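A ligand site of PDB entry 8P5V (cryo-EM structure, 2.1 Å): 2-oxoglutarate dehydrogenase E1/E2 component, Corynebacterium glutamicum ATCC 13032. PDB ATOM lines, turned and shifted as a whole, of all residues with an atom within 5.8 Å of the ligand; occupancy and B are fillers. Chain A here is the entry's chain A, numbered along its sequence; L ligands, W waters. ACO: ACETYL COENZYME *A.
Water W8 lies within hydrogen-bond range of an oxygen (O1A) of the ligand (2.5 Å) and the guanidinium group (NH1) of Arg 1053 (2.7 Å). Water W2 lies within hydrogen-bond range of an oxygen (O3B) of the ligand (2.6 Å) and the backbone carbonyl oxygen (O) of Pro 830 (2.6 Å). Water W7 lies within hydrogen-bond range of an oxygen (O9P) of the ligand (2.7 Å) and the side-chain amide nitrogen of Asn 1145 (3.0 Å). Water W4 lies within hydrogen-bond range of the backbone carbonyl oxygen of Phe 1090, an oxygen (O1A) of the ligand and the backbone NH of Ser 1092.
The guanidinium group of Arg 1053 lies within hydrogen-bond range of the side-chain sulfur of Met 1138, 3.7 Å away. The guanidinium group (NH1) of Arg 1061 sits at hydrogen-bond distance from the backbone carbonyl oxygen (O) of Thr 824. A ring nitrogen (ND1) of His 1140 is in hydrogen-bond range of the backbone carbonyl oxygen of Met 1036 (2.9 Å). The backbone carbonyl oxygen (O) of Arg 1053 is in hydrogen-bond range of the side-chain hydroxyl (OG) of Ser 1057, at 3.1 Å. NZ of Lys 1089 lies within hydrogen-bond range of O of Leu 833 (2.7 Å). O of Ser 1092 lies within hydrogen-bond range of N of Met 1138 (3.3 Å). The guanidinium group (NH1) of Arg 1061 sits close to the backbone carbonyl oxygen (O) of Gly 1034, at 3.0 Å.
The side-chain sulfur (SD) of Met 1138 sits close to a nitrogen (N7A) of the ligand. O of Pro 1143 sits close to O4A of the ligand, at 3.3 Å. Thr 824 touches the ligand (CG2 to O5P, 3.6 Å). CD2 of Leu 829 touches O of the ligand (3.7 Å). CD of Pro 830 touches N3A of the ligand, at 3.4 Å. O of Gly 1034 touches CH3 of the ligand, 3.2 Å away. Met 1036 touches the ligand (O to CH3, 3.999 Å). Leu 1059 touches the ligand (CD2 to N1A, 3.6 Å). Pro 1141 touches the ligand. Phe 1144 touches the ligand (N to O4A, 3.5 Å). The nearest printed residue that does not touch the ligand is Leu 833 (4.4 Å).
ND2 of Asn 1145 lies within hydrogen-bond range of O5A of the ligand, at 3.2 Å. N of Gly 832 lies within hydrogen-bond range of O8A of the ligand (2.9 Å). ND1 of His 831 sits at hydrogen-bond distance from O7A of the ligand. O8A of the ligand is in salt-bridge range of NZ of Lys 1089 (2.9 Å). N of Asn 1145 is in hydrogen-bond range of O4A of the ligand (3.0 Å). NH1 of Arg 1053 is in hydrogen-bond range of O2B of the ligand (3.0 Å). N6A of the ligand is in hydrogen-bond range of OG1 of Thr 1037. O2A of the ligand is in salt-bridge range of NH1 of Arg 1146, at 2.6 Å. NH1 of Arg 1061 lies close to S1P of the ligand (3.4 Å). OG of Ser 1092 lies within hydrogen-bond range of O1A of the ligand. An oxygen (O4A) of the ligand is in hydrogen-bond range of the backbone NH (N) of Arg 1146 (3.0 Å). The backbone carbonyl oxygen (O) of Ile 1142 sits at hydrogen-bond distance from an oxygen (OAP) of the ligand (2.7 Å).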
ATOM      1  N   THR A 824      38.698  10.102  -7.084  1.00  0.00           N
ATOM      2  CA  THR A 824      37.568   9.853  -7.961  1.00  0.00           C
ATOM      3  C   THR A 824      37.470   8.360  -8.273  1.00  0.00           C
ATOM      4  O   THR A 824      36.404   7.759  -8.104  1.00  0.00           O
ATOM      5  CB  THR A 824      37.646  10.691  -9.238  1.00  0.00           C
ATOM      6  OG1 THR A 824      37.895  12.045  -8.872  1.00  0.00           O
ATOM      7  CG2 THR A 824      36.395  10.602 -10.085  1.00  0.00           C
ATOM      8  N   LEU A 829      32.882   1.225  -9.303  1.00  0.00           N
ATOM      9  CA  LEU A 829      31.433   1.220  -9.462  1.00  0.00           C
ATOM     10  C   LEU A 829      30.953  -0.212  -9.683  1.00  0.00           C
ATOM     11  O   LEU A 829      31.620  -0.985 -10.369  1.00  0.00           O
ATOM     12  CB  LEU A 829      31.047   2.113 -10.643  1.00  0.00           C
ATOM     13  CG  LEU A 829      31.250   3.612 -10.459  1.00  0.00           C
ATOM     14  CD1 LEU A 829      30.680   4.378 -11.640  1.00  0.00           C
ATOM     15  CD2 LEU A 829      30.621   4.109  -9.168  1.00  0.00           C
ATOM     16  N   PRO A 830      29.793  -0.597  -9.124  1.00  0.00           N
ATOM     17  CA  PRO A 830      29.238  -1.941  -9.310  1.00  0.00           C
ATOM     18  C   PRO A 830      28.606  -2.163 -10.681  1.00  0.00           C
ATOM     19  O   PRO A 830      27.388  -2.119 -10.823  1.00  0.00           O
ATOM     20  CB  PRO A 830      28.183  -2.018  -8.202  1.00  0.00           C
ATOM     21  CG  PRO A 830      27.688  -0.593  -8.094  1.00  0.00           C
ATOM     22  CD  PRO A 830      28.929   0.247  -8.278  1.00  0.00           C
ATOM     23  N   HIS A 831      29.448  -2.402 -11.689  1.00  0.00           N
ATOM     24  CA  HIS A 831      28.978  -2.674 -13.040  1.00  0.00           C
ATOM     25  C   HIS A 831      28.407  -4.084 -13.113  1.00  0.00           C
ATOM     26  O   HIS A 831      29.041  -5.031 -12.664  1.00  0.00           O
ATOM     27  CB  HIS A 831      30.113  -2.469 -14.055  1.00  0.00           C
ATOM     28  CG  HIS A 831      30.543  -1.046 -14.172  1.00  0.00           C
ATOM     29  ND1 HIS A 831      29.720  -0.069 -14.679  1.00  0.00           N
ATOM     30  CD2 HIS A 831      31.696  -0.446 -13.843  1.00  0.00           C
ATOM     31  CE1 HIS A 831      30.365   1.092 -14.661  1.00  0.00           C
ATOM     32  NE2 HIS A 831      31.559   0.883 -14.148  1.00  0.00           N
ATOM     33  N   GLY A 832      27.199  -4.198 -13.659  1.00  0.00           N
ATOM     34  CA  GLY A 832      26.570  -5.487 -13.900  1.00  0.00           C
ATOM     35  C   GLY A 832      25.739  -5.989 -12.717  1.00  0.00           C
ATOM     36  O   GLY A 832      25.180  -7.080 -12.790  1.00  0.00           O
ATOM     37  N   LEU A 833      25.646  -5.187 -11.656  1.00  0.00           N
ATOM     38  CA  LEU A 833      24.935  -5.601 -10.453  1.00  0.00           C
ATOM     39  C   LEU A 833      23.435  -5.469 -10.683  1.00  0.00           C
ATOM     40  O   LEU A 833      22.960  -4.428 -11.143  1.00  0.00           O
ATOM     41  CB  LEU A 833      25.383  -4.740  -9.270  1.00  0.00           C
ATOM     42  CG  LEU A 833      24.663  -5.004  -7.959  1.00  0.00           C
ATOM     43  CD1 LEU A 833      25.028  -6.369  -7.402  1.00  0.00           C
ATOM     44  CD2 LEU A 833      24.987  -3.921  -6.943  1.00  0.00           C
ATOM     45  N   GLU A1033      34.960  15.086  -6.878  1.00  0.00           N
ATOM     46  CA  GLU A1033      35.709  13.854  -7.079  1.00  0.00           C
ATOM     47  C   GLU A1033      34.876  12.647  -6.656  1.00  0.00           C
ATOM     48  O   GLU A1033      35.380  11.718  -6.029  1.00  0.00           O
ATOM     49  CB  GLU A1033      37.044  13.874  -6.313  1.00  0.00           C
ATOM     50  CG  GLU A1033      37.694  15.235  -6.174  1.00  0.00           C
ATOM     51  CD  GLU A1033      38.778  15.294  -5.104  1.00  0.00           C
ATOM     52  OE1 GLU A1033      38.478  14.964  -3.936  1.00  0.00           O
ATOM     53  OE2 GLU A1033      39.918  15.680  -5.438  1.00  0.00           O
ATOM     54  N   GLY A1034      33.584  12.644  -7.011  1.00  0.00           N
ATOM     55  CA  GLY A1034      32.687  11.542  -6.732  1.00  0.00           C
ATOM     56  C   GLY A1034      32.591  11.195  -5.250  1.00  0.00           C
ATOM     57  O   GLY A1034      32.591  10.025  -4.899  1.00  0.00           O
ATOM     58  N   SER A1035      32.501  12.220  -4.395  1.00  0.00           N
ATOM     59  CA  SER A1035      32.566  12.044  -2.946  1.00  0.00           C
ATOM     60  C   SER A1035      31.355  11.280  -2.418  1.00  0.00           C
ATOM     61  O   SER A1035      31.494  10.444  -1.524  1.00  0.00           O
ATOM     62  CB  SER A1035      32.676  13.369  -2.258  1.00  0.00           C
ATOM     63  OG  SER A1035      33.947  13.953  -2.489  1.00  0.00           O
ATOM     64  N   MET A1036      30.149  11.598  -2.923  1.00  0.00           N
ATOM     65  CA  MET A1036      28.940  10.930  -2.478  1.00  0.00           C
ATOM     66  C   MET A1036      27.905  10.923  -3.599  1.00  0.00           C
ATOM     67  O   MET A1036      28.023  11.663  -4.567  1.00  0.00           O
ATOM     68  CB  MET A1036      28.344  11.596  -1.235  1.00  0.00           C
ATOM     69  CG  MET A1036      28.650  13.064  -1.102  1.00  0.00           C
ATOM     70  SD  MET A1036      28.066  13.763   0.468  1.00  0.00           S
ATOM     71  CE  MET A1036      27.825  15.478  -0.022  1.00  0.00           C
ATOM     72  N   THR A1037      26.904  10.054  -3.438  1.00  0.00           N
ATOM     73  CA  THR A1037      25.798   9.952  -4.370  1.00  0.00           C
ATOM     74  C   THR A1037      24.647  10.819  -3.861  1.00  0.00           C
ATOM     75  O   THR A1037      24.285  10.716  -2.694  1.00  0.00           O
ATOM     76  CB  THR A1037      25.365   8.496  -4.566  1.00  0.00           C
ATOM     77  OG1 THR A1037      26.500   7.701  -4.914  1.00  0.00           O
ATOM     78  CG2 THR A1037      24.310   8.339  -5.640  1.00  0.00           C
ATOM     79  N   ARG A1053      21.290  -0.974  -4.623  1.00  0.00           N
ATOM     80  CA  ARG A1053      22.550  -0.810  -5.335  1.00  0.00           C
ATOM     81  C   ARG A1053      23.619  -0.329  -4.349  1.00  0.00           C
ATOM     82  O   ARG A1053      24.733  -0.839  -4.355  1.00  0.00           O
ATOM     83  CB  ARG A1053      22.416   0.171  -6.491  1.00  0.00           C
ATOM     84  CG  ARG A1053      23.660   0.258  -7.363  1.00  0.00           C
ATOM     85  CD  ARG A1053      23.526   1.250  -8.499  1.00  0.00           C
ATOM     86  NE  ARG A1053      23.424   2.613  -8.026  1.00  0.00           N
ATOM     87  CZ  ARG A1053      23.354   3.681  -8.805  1.00  0.00           C
ATOM     88  NH1 ARG A1053      23.410   3.538 -10.128  1.00  0.00           N
ATOM     89  NH2 ARG A1053      23.227   4.880  -8.282  1.00  0.00           N
ATOM     90  N   SER A1057      26.815  -2.931  -3.203  1.00  0.00           N
ATOM     91  CA  SER A1057      28.015  -2.575  -3.937  1.00  0.00           C
ATOM     92  C   SER A1057      29.231  -2.529  -3.014  1.00  0.00           C
ATOM     93  O   SER A1057      29.090  -2.671  -1.796  1.00  0.00           O
ATOM     94  CB  SER A1057      27.856  -1.259  -4.646  1.00  0.00           C
ATOM     95  OG  SER A1057      27.687  -0.211  -3.706  1.00  0.00           O
ATOM     96  N   LEU A1059      31.150   0.230  -3.320  1.00  0.00           N
ATOM     97  CA  LEU A1059      31.401   1.668  -3.311  1.00  0.00           C
ATOM     98  C   LEU A1059      31.045   2.222  -1.933  1.00  0.00           C
ATOM     99  O   LEU A1059      29.887   2.512  -1.647  1.00  0.00           O
ATOM    100  CB  LEU A1059      30.579   2.319  -4.420  1.00  0.00           C
ATOM    101  CG  LEU A1059      30.795   3.830  -4.600  1.00  0.00           C
ATOM    102  CD1 LEU A1059      32.184   4.127  -5.113  1.00  0.00           C
ATOM    103  CD2 LEU A1059      29.748   4.405  -5.540  1.00  0.00           C
ATOM    104  N   ARG A1061      30.751   4.917  -0.101  1.00  0.00           N
ATOM    105  CA  ARG A1061      30.578   6.354  -0.074  1.00  0.00           C
ATOM    106  C   ARG A1061      29.155   6.678   0.345  1.00  0.00           C
ATOM    107  O   ARG A1061      28.251   5.889   0.110  1.00  0.00           O
ATOM    108  CB  ARG A1061      30.898   6.939  -1.453  1.00  0.00           C
ATOM    109  CG  ARG A1061      32.351   6.784  -1.843  1.00  0.00           C
ATOM    110  CD  ARG A1061      32.733   7.630  -3.041  1.00  0.00           C
ATOM    111  NE  ARG A1061      34.181   7.687  -3.174  1.00  0.00           N
ATOM    112  CZ  ARG A1061      34.844   7.558  -4.315  1.00  0.00           C
ATOM    113  NH1 ARG A1061      34.208   7.503  -5.471  1.00  0.00           N
ATOM    114  NH2 ARG A1061      36.169   7.531  -4.281  1.00  0.00           N
ATOM    115  N   LYS A1089      17.810  -2.911 -12.659  1.00  0.00           N
ATOM    116  CA  LYS A1089      18.751  -1.876 -12.248  1.00  0.00           C
ATOM    117  C   LYS A1089      18.020  -0.581 -11.916  1.00  0.00           C
ATOM    118  O   LYS A1089      16.941  -0.308 -12.426  1.00  0.00           O
ATOM    119  CB  LYS A1089      19.777  -1.642 -13.358  1.00  0.00           C
ATOM    120  CG  LYS A1089      20.705  -2.812 -13.630  1.00  0.00           C
ATOM    121  CD  LYS A1089      21.657  -2.563 -14.782  1.00  0.00           C
ATOM    122  CE  LYS A1089      22.679  -3.667 -14.950  1.00  0.00           C
ATOM    123  NZ  LYS A1089      23.527  -3.786 -13.752  1.00  0.00           N
ATOM    124  N   PHE A1090      18.649   0.223 -11.047  1.00  0.00           N
ATOM    125  CA  PHE A1090      18.255   1.601 -10.798  1.00  0.00           C
ATOM    126  C   PHE A1090      18.385   2.414 -12.082  1.00  0.00           C
ATOM    127  O   PHE A1090      19.305   2.209 -12.859  1.00  0.00           O
ATOM    128  CB  PHE A1090      19.138   2.206  -9.708  1.00  0.00           C
ATOM    129  CG  PHE A1090      19.054   3.697  -9.575  1.00  0.00           C
ATOM    130  CD1 PHE A1090      17.981   4.285  -8.911  1.00  0.00           C
ATOM    131  CD2 PHE A1090      20.017   4.519 -10.136  1.00  0.00           C
ATOM    132  CE1 PHE A1090      17.897   5.668  -8.790  1.00  0.00           C
ATOM    133  CE2 PHE A1090      19.924   5.898 -10.017  1.00  0.00           C
ATOM    134  CZ  PHE A1090      18.873   6.467  -9.340  1.00  0.00           C
ATOM    135  N   SER A1092      18.963   6.111 -13.524  1.00  0.00           N
ATOM    136  CA  SER A1092      19.446   7.439 -13.217  1.00  0.00           C
ATOM    137  C   SER A1092      18.652   8.486 -13.988  1.00  0.00           C
ATOM    138  O   SER A1092      18.464   9.606 -13.508  1.00  0.00           O
ATOM    139  CB  SER A1092      20.919   7.553 -13.489  1.00  0.00           C
ATOM    140  OG  SER A1092      21.198   7.263 -14.851  1.00  0.00           O
ATOM    141  N   MET A1138      19.243  10.661 -10.428  1.00  0.00           N
ATOM    142  CA  MET A1138      20.515  10.783  -9.738  1.00  0.00           C
ATOM    143  C   MET A1138      21.149  12.120 -10.130  1.00  0.00           C
ATOM    144  O   MET A1138      21.416  12.354 -11.304  1.00  0.00           O
ATOM    145  CB  MET A1138      21.448   9.632 -10.103  1.00  0.00           C
ATOM    146  CG  MET A1138      22.791   9.693  -9.390  1.00  0.00           C
ATOM    147  SD  MET A1138      23.841   8.251  -9.693  1.00  0.00           S
ATOM    148  CE  MET A1138      24.271   8.504 -11.409  1.00  0.00           C
ATOM    149  N   HIS A1140      24.025  13.730  -8.477  1.00  0.00           N
ATOM    150  CA  HIS A1140      25.474  13.562  -8.489  1.00  0.00           C
ATOM    151  C   HIS A1140      25.806  12.104  -8.206  1.00  0.00           C
ATOM    152  O   HIS A1140      25.287  11.540  -7.241  1.00  0.00           O
ATOM    153  CB  HIS A1140      26.136  14.469  -7.449  1.00  0.00           C
ATOM    154  CG  HIS A1140      27.619  14.390  -7.496  1.00  0.00           C
ATOM    155  ND1 HIS A1140      28.359  13.633  -6.608  1.00  0.00           N
ATOM    156  CD2 HIS A1140      28.503  14.936  -8.350  1.00  0.00           C
ATOM    157  CE1 HIS A1140      29.650  13.741  -6.915  1.00  0.00           C
ATOM    158  NE2 HIS A1140      29.749  14.533  -7.960  1.00  0.00           N
ATOM    159  N   PRO A1141      26.682  11.431  -8.997  1.00  0.00           N
ATOM    160  CA  PRO A1141      27.298  12.008 -10.194  1.00  0.00           C
ATOM    161  C   PRO A1141      26.285  12.297 -11.294  1.00  0.00           C
ATOM    162  O   PRO A1141      25.198  11.739 -11.289  1.00  0.00           O
ATOM    163  CB  PRO A1141      28.262  10.922 -10.688  1.00  0.00           C
ATOM    164  CG  PRO A1141      28.406   9.962  -9.524  1.00  0.00           C
ATOM    165  CD  PRO A1141      27.099  10.044  -8.769  1.00  0.00           C
ATOM    166  N   ILE A1142      26.659  13.171 -12.226  1.00  0.00           N
ATOM    167  CA  ILE A1142      25.789  13.554 -13.321  1.00  0.00           C
ATOM    168  C   ILE A1142      25.776  12.418 -14.336  1.00  0.00           C
ATOM    169  O   ILE A1142      26.809  12.065 -14.884  1.00  0.00           O
ATOM    170  CB  ILE A1142      26.252  14.879 -13.973  1.00  0.00           C
ATOM    171  CG1 ILE A1142      26.322  16.020 -12.959  1.00  0.00           C
ATOM    172  CG2 ILE A1142      25.360  15.230 -15.156  1.00  0.00           C
ATOM    173  CD1 ILE A1142      26.962  17.278 -13.492  1.00  0.00           C
ATOM    174  N   PRO A1143      24.600  11.829 -14.644  1.00  0.00           N
ATOM    175  CA  PRO A1143      24.500  10.797 -15.679  1.00  0.00           C
ATOM    176  C   PRO A1143      24.397  11.389 -17.075  1.00  0.00           C
ATOM    177  O   PRO A1143      23.377  11.259 -17.734  1.00  0.00           O
ATOM    178  CB  PRO A1143      23.235  10.057 -15.267  1.00  0.00           C
ATOM    179  CG  PRO A1143      22.351  11.143 -14.688  1.00  0.00           C
ATOM    180  CD  PRO A1143      23.310  12.082 -13.987  1.00  0.00           C
ATOM    181  N   PHE A1144      25.491  12.014 -17.529  1.00  0.00           N
ATOM    182  CA  PHE A1144      25.479  12.789 -18.757  1.00  0.00           C
ATOM    183  C   PHE A1144      25.356  11.887 -19.981  1.00  0.00           C
ATOM    184  O   PHE A1144      24.835  12.324 -21.004  1.00  0.00           O
ATOM    185  CB  PHE A1144      26.718  13.699 -18.850  1.00  0.00           C
ATOM    186  CG  PHE A1144      28.037  13.004 -18.802  1.00  0.00           C
ATOM    187  CD1 PHE A1144      28.682  12.766 -17.591  1.00  0.00           C
ATOM    188  CD2 PHE A1144      28.663  12.567 -19.968  1.00  0.00           C
ATOM    189  CE1 PHE A1144      29.907  12.127 -17.551  1.00  0.00           C
ATOM    190  CE2 PHE A1144      29.880  11.917 -19.916  1.00  0.00           C
ATOM    191  CZ  PHE A1144      30.504  11.693 -18.706  1.00  0.00           C
ATOM    192  N   ASN A1145      25.829  10.639 -19.883  1.00  0.00           N
ATOM    193  CA  ASN A1145      25.699   9.687 -20.974  1.00  0.00           C
ATOM    194  C   ASN A1145      24.223   9.346 -21.180  1.00  0.00           C
ATOM    195  O   ASN A1145      23.756   9.305 -22.320  1.00  0.00           O
ATOM    196  CB  ASN A1145      26.531   8.421 -20.735  1.00  0.00           C
ATOM    197  CG  ASN A1145      28.014   8.697 -20.719  1.00  0.00           C
ATOM    198  OD1 ASN A1145      28.550   9.234 -21.680  1.00  0.00           O
ATOM    199  ND2 ASN A1145      28.690   8.337 -19.638  1.00  0.00           N
ATOM    200  N   ARG A1146      23.500   9.133 -20.084  1.00  0.00           N
ATOM    201  CA  ARG A1146      22.092   8.812 -20.148  1.00  0.00           C
ATOM    202  C   ARG A1146      21.284  10.032 -20.609  1.00  0.00           C
ATOM    203  O   ARG A1146      20.342   9.873 -21.385  1.00  0.00           O
ATOM    204  CB  ARG A1146      21.578   8.326 -18.783  1.00  0.00           C
ATOM    205  CG  ARG A1146      22.203   7.029 -18.303  1.00  0.00           C
ATOM    206  CD  ARG A1146      21.754   5.808 -19.082  1.00  0.00           C
ATOM    207  NE  ARG A1146      22.380   5.674 -20.391  1.00  0.00           N
ATOM    208  CZ  ARG A1146      23.675   5.426 -20.593  1.00  0.00           C
ATOM    209  NH1 ARG A1146      24.494   5.255 -19.568  1.00  0.00           N
ATOM    210  NH2 ARG A1146      24.135   5.340 -21.823  1.00  0.00           N
ATOM    211  N   ILE A1147      21.657  11.220 -20.136  1.00  0.00           N
ATOM    212  CA  ILE A1147      20.982  12.452 -20.517  1.00  0.00           C
ATOM    213  C   ILE A1147      21.221  12.711 -22.009  1.00  0.00           C
ATOM    214  O   ILE A1147      20.307  13.103 -22.713  1.00  0.00           O
ATOM    215  CB  ILE A1147      21.422  13.641 -19.643  1.00  0.00           C
ATOM    216  CG1 ILE A1147      21.021  13.453 -18.178  1.00  0.00           C
ATOM    217  CG2 ILE A1147      20.877  14.947 -20.195  1.00  0.00           C
ATOM    218  CD1 ILE A1147      21.693  14.410 -17.226  1.00  0.00           C
HETATM  219  N1A ACO L   1      26.640   4.172  -7.348  1.00  0.00           N
HETATM  220  C2A ACO L   1      26.685   2.964  -7.922  1.00  0.00           C
HETATM  221  N3A ACO L   1      26.723   2.658  -9.227  1.00  0.00           N
HETATM  222  C4A ACO L   1      26.688   3.758  -9.980  1.00  0.00           C
HETATM  223  C5A ACO L   1      26.636   5.070  -9.539  1.00  0.00           C
HETATM  224  C6A ACO L   1      26.614   5.269  -8.142  1.00  0.00           C
HETATM  225  N6A ACO L   1      26.560   6.471  -7.570  1.00  0.00           N
HETATM  226  N7A ACO L   1      26.598   5.949 -10.606  1.00  0.00           N
HETATM  227  C8A ACO L   1      26.627   5.169 -11.654  1.00  0.00           C
HETATM  228  N9A ACO L   1      26.678   3.826 -11.356  1.00  0.00           N
HETATM  229  C1B ACO L   1      26.667   2.719 -12.290  1.00  0.00           C
HETATM  230  C2B ACO L   1      25.291   2.368 -12.799  1.00  0.00           C
HETATM  231  O2B ACO L   1      24.677   1.446 -11.899  1.00  0.00           O
HETATM  232  C3B ACO L   1      25.633   1.734 -14.147  1.00  0.00           C
HETATM  233  O3B ACO L   1      25.938   0.342 -14.004  1.00  0.00           O
HETATM  234  P3B ACO L   1      25.818  -0.641 -15.293  1.00  0.00           P
HETATM  235  O7A ACO L   1      27.120  -0.490 -16.051  1.00  0.00           O
HETATM  236  O8A ACO L   1      25.661  -2.005 -14.657  1.00  0.00           O
HETATM  237  O9A ACO L   1      24.607  -0.209 -16.088  1.00  0.00           O
HETATM  238  C4B ACO L   1      26.839   2.546 -14.624  1.00  0.00           C
HETATM  239  O4B ACO L   1      27.437   3.076 -13.421  1.00  0.00           O
HETATM  240  C5B ACO L   1      26.543   3.662 -15.581  1.00  0.00           C
HETATM  241  O5B ACO L   1      25.716   4.651 -14.907  1.00  0.00           O
HETATM  242  P1A ACO L   1      24.591   5.481 -15.674  1.00  0.00           P
HETATM  243  O1A ACO L   1      23.488   5.675 -14.719  1.00  0.00           O
HETATM  244  O2A ACO L   1      24.312   4.910 -17.010  1.00  0.00           O
HETATM  245  O3A ACO L   1      25.331   6.892 -15.859  1.00  0.00           O
HETATM  246  P2A ACO L   1      26.150   7.517 -17.082  1.00  0.00           P
HETATM  247  O4A ACO L   1      25.306   8.521 -17.760  1.00  0.00           O
HETATM  248  O5A ACO L   1      26.782   6.432 -17.857  1.00  0.00           O
HETATM  249  O6A ACO L   1      27.288   8.286 -16.298  1.00  0.00           O
HETATM  250  CBP ACO L   1      28.655   8.324 -14.306  1.00  0.00           C
HETATM  251  CCP ACO L   1      28.299   7.571 -15.574  1.00  0.00           C
HETATM  252  CDP ACO L   1      29.696   7.539 -13.507  1.00  0.00           C
HETATM  253  CEP ACO L   1      27.371   8.459 -13.469  1.00  0.00           C
HETATM  254  CAP ACO L   1      29.187   9.722 -14.688  1.00  0.00           C
HETATM  255  OAP ACO L   1      28.816  10.700 -13.716  1.00  0.00           O
HETATM  256  C9P ACO L   1      30.696   9.796 -14.880  1.00  0.00           C
HETATM  257  O9P ACO L   1      31.214   9.329 -15.889  1.00  0.00           O
HETATM  258  N8P ACO L   1      31.385  10.383 -13.914  1.00  0.00           N
HETATM  259  C7P ACO L   1      32.833  10.520 -13.937  1.00  0.00           C
HETATM  260  C6P ACO L   1      33.371  11.113 -12.642  1.00  0.00           C
HETATM  261  C5P ACO L   1      33.044  10.286 -11.418  1.00  0.00           C
HETATM  262  O5P ACO L   1      32.813  10.831 -10.345  1.00  0.00           O
HETATM  263  N4P ACO L   1      33.015   8.958 -11.575  1.00  0.00           N
HETATM  264  C3P ACO L   1      32.848   8.044 -10.453  1.00  0.00           C
HETATM  265  C2P ACO L   1      31.529   8.165  -9.703  1.00  0.00           C
HETATM  266  S1P ACO L   1      31.827   7.853  -7.937  1.00  0.00           S
HETATM  267  C   ACO L   1      30.152   7.825  -7.344  1.00  0.00           C
HETATM  268  O   ACO L   1      29.260   7.315  -7.956  1.00  0.00           O
HETATM  269  CH3 ACO L   1      29.993   8.499  -6.016  1.00  0.00           C
HETATM  270  O   HOH W   1      22.132   0.590 -15.551  1.00  0.00           O
HETATM  271  O   HOH W   2      25.336  -1.100 -11.985  1.00  0.00           O
HETATM  272  O   HOH W   3      25.811   3.872  -4.838  1.00  0.00           O
HETATM  273  O   HOH W   4      21.125   3.930 -14.188  1.00  0.00           O
HETATM  274  O   HOH W   5      27.602   1.462 -17.788  1.00  0.00           O
HETATM  275  O   HOH W   6      33.298   6.319 -13.284  1.00  0.00           O
HETATM  276  O   HOH W   7      31.482   8.527 -18.491  1.00  0.00           O
HETATM  277  O   HOH W   8      23.094   5.181 -12.254  1.00  0.00           O
HETATM  278  O   HOH W   9      28.734   4.650 -18.140  1.00  0.00           O
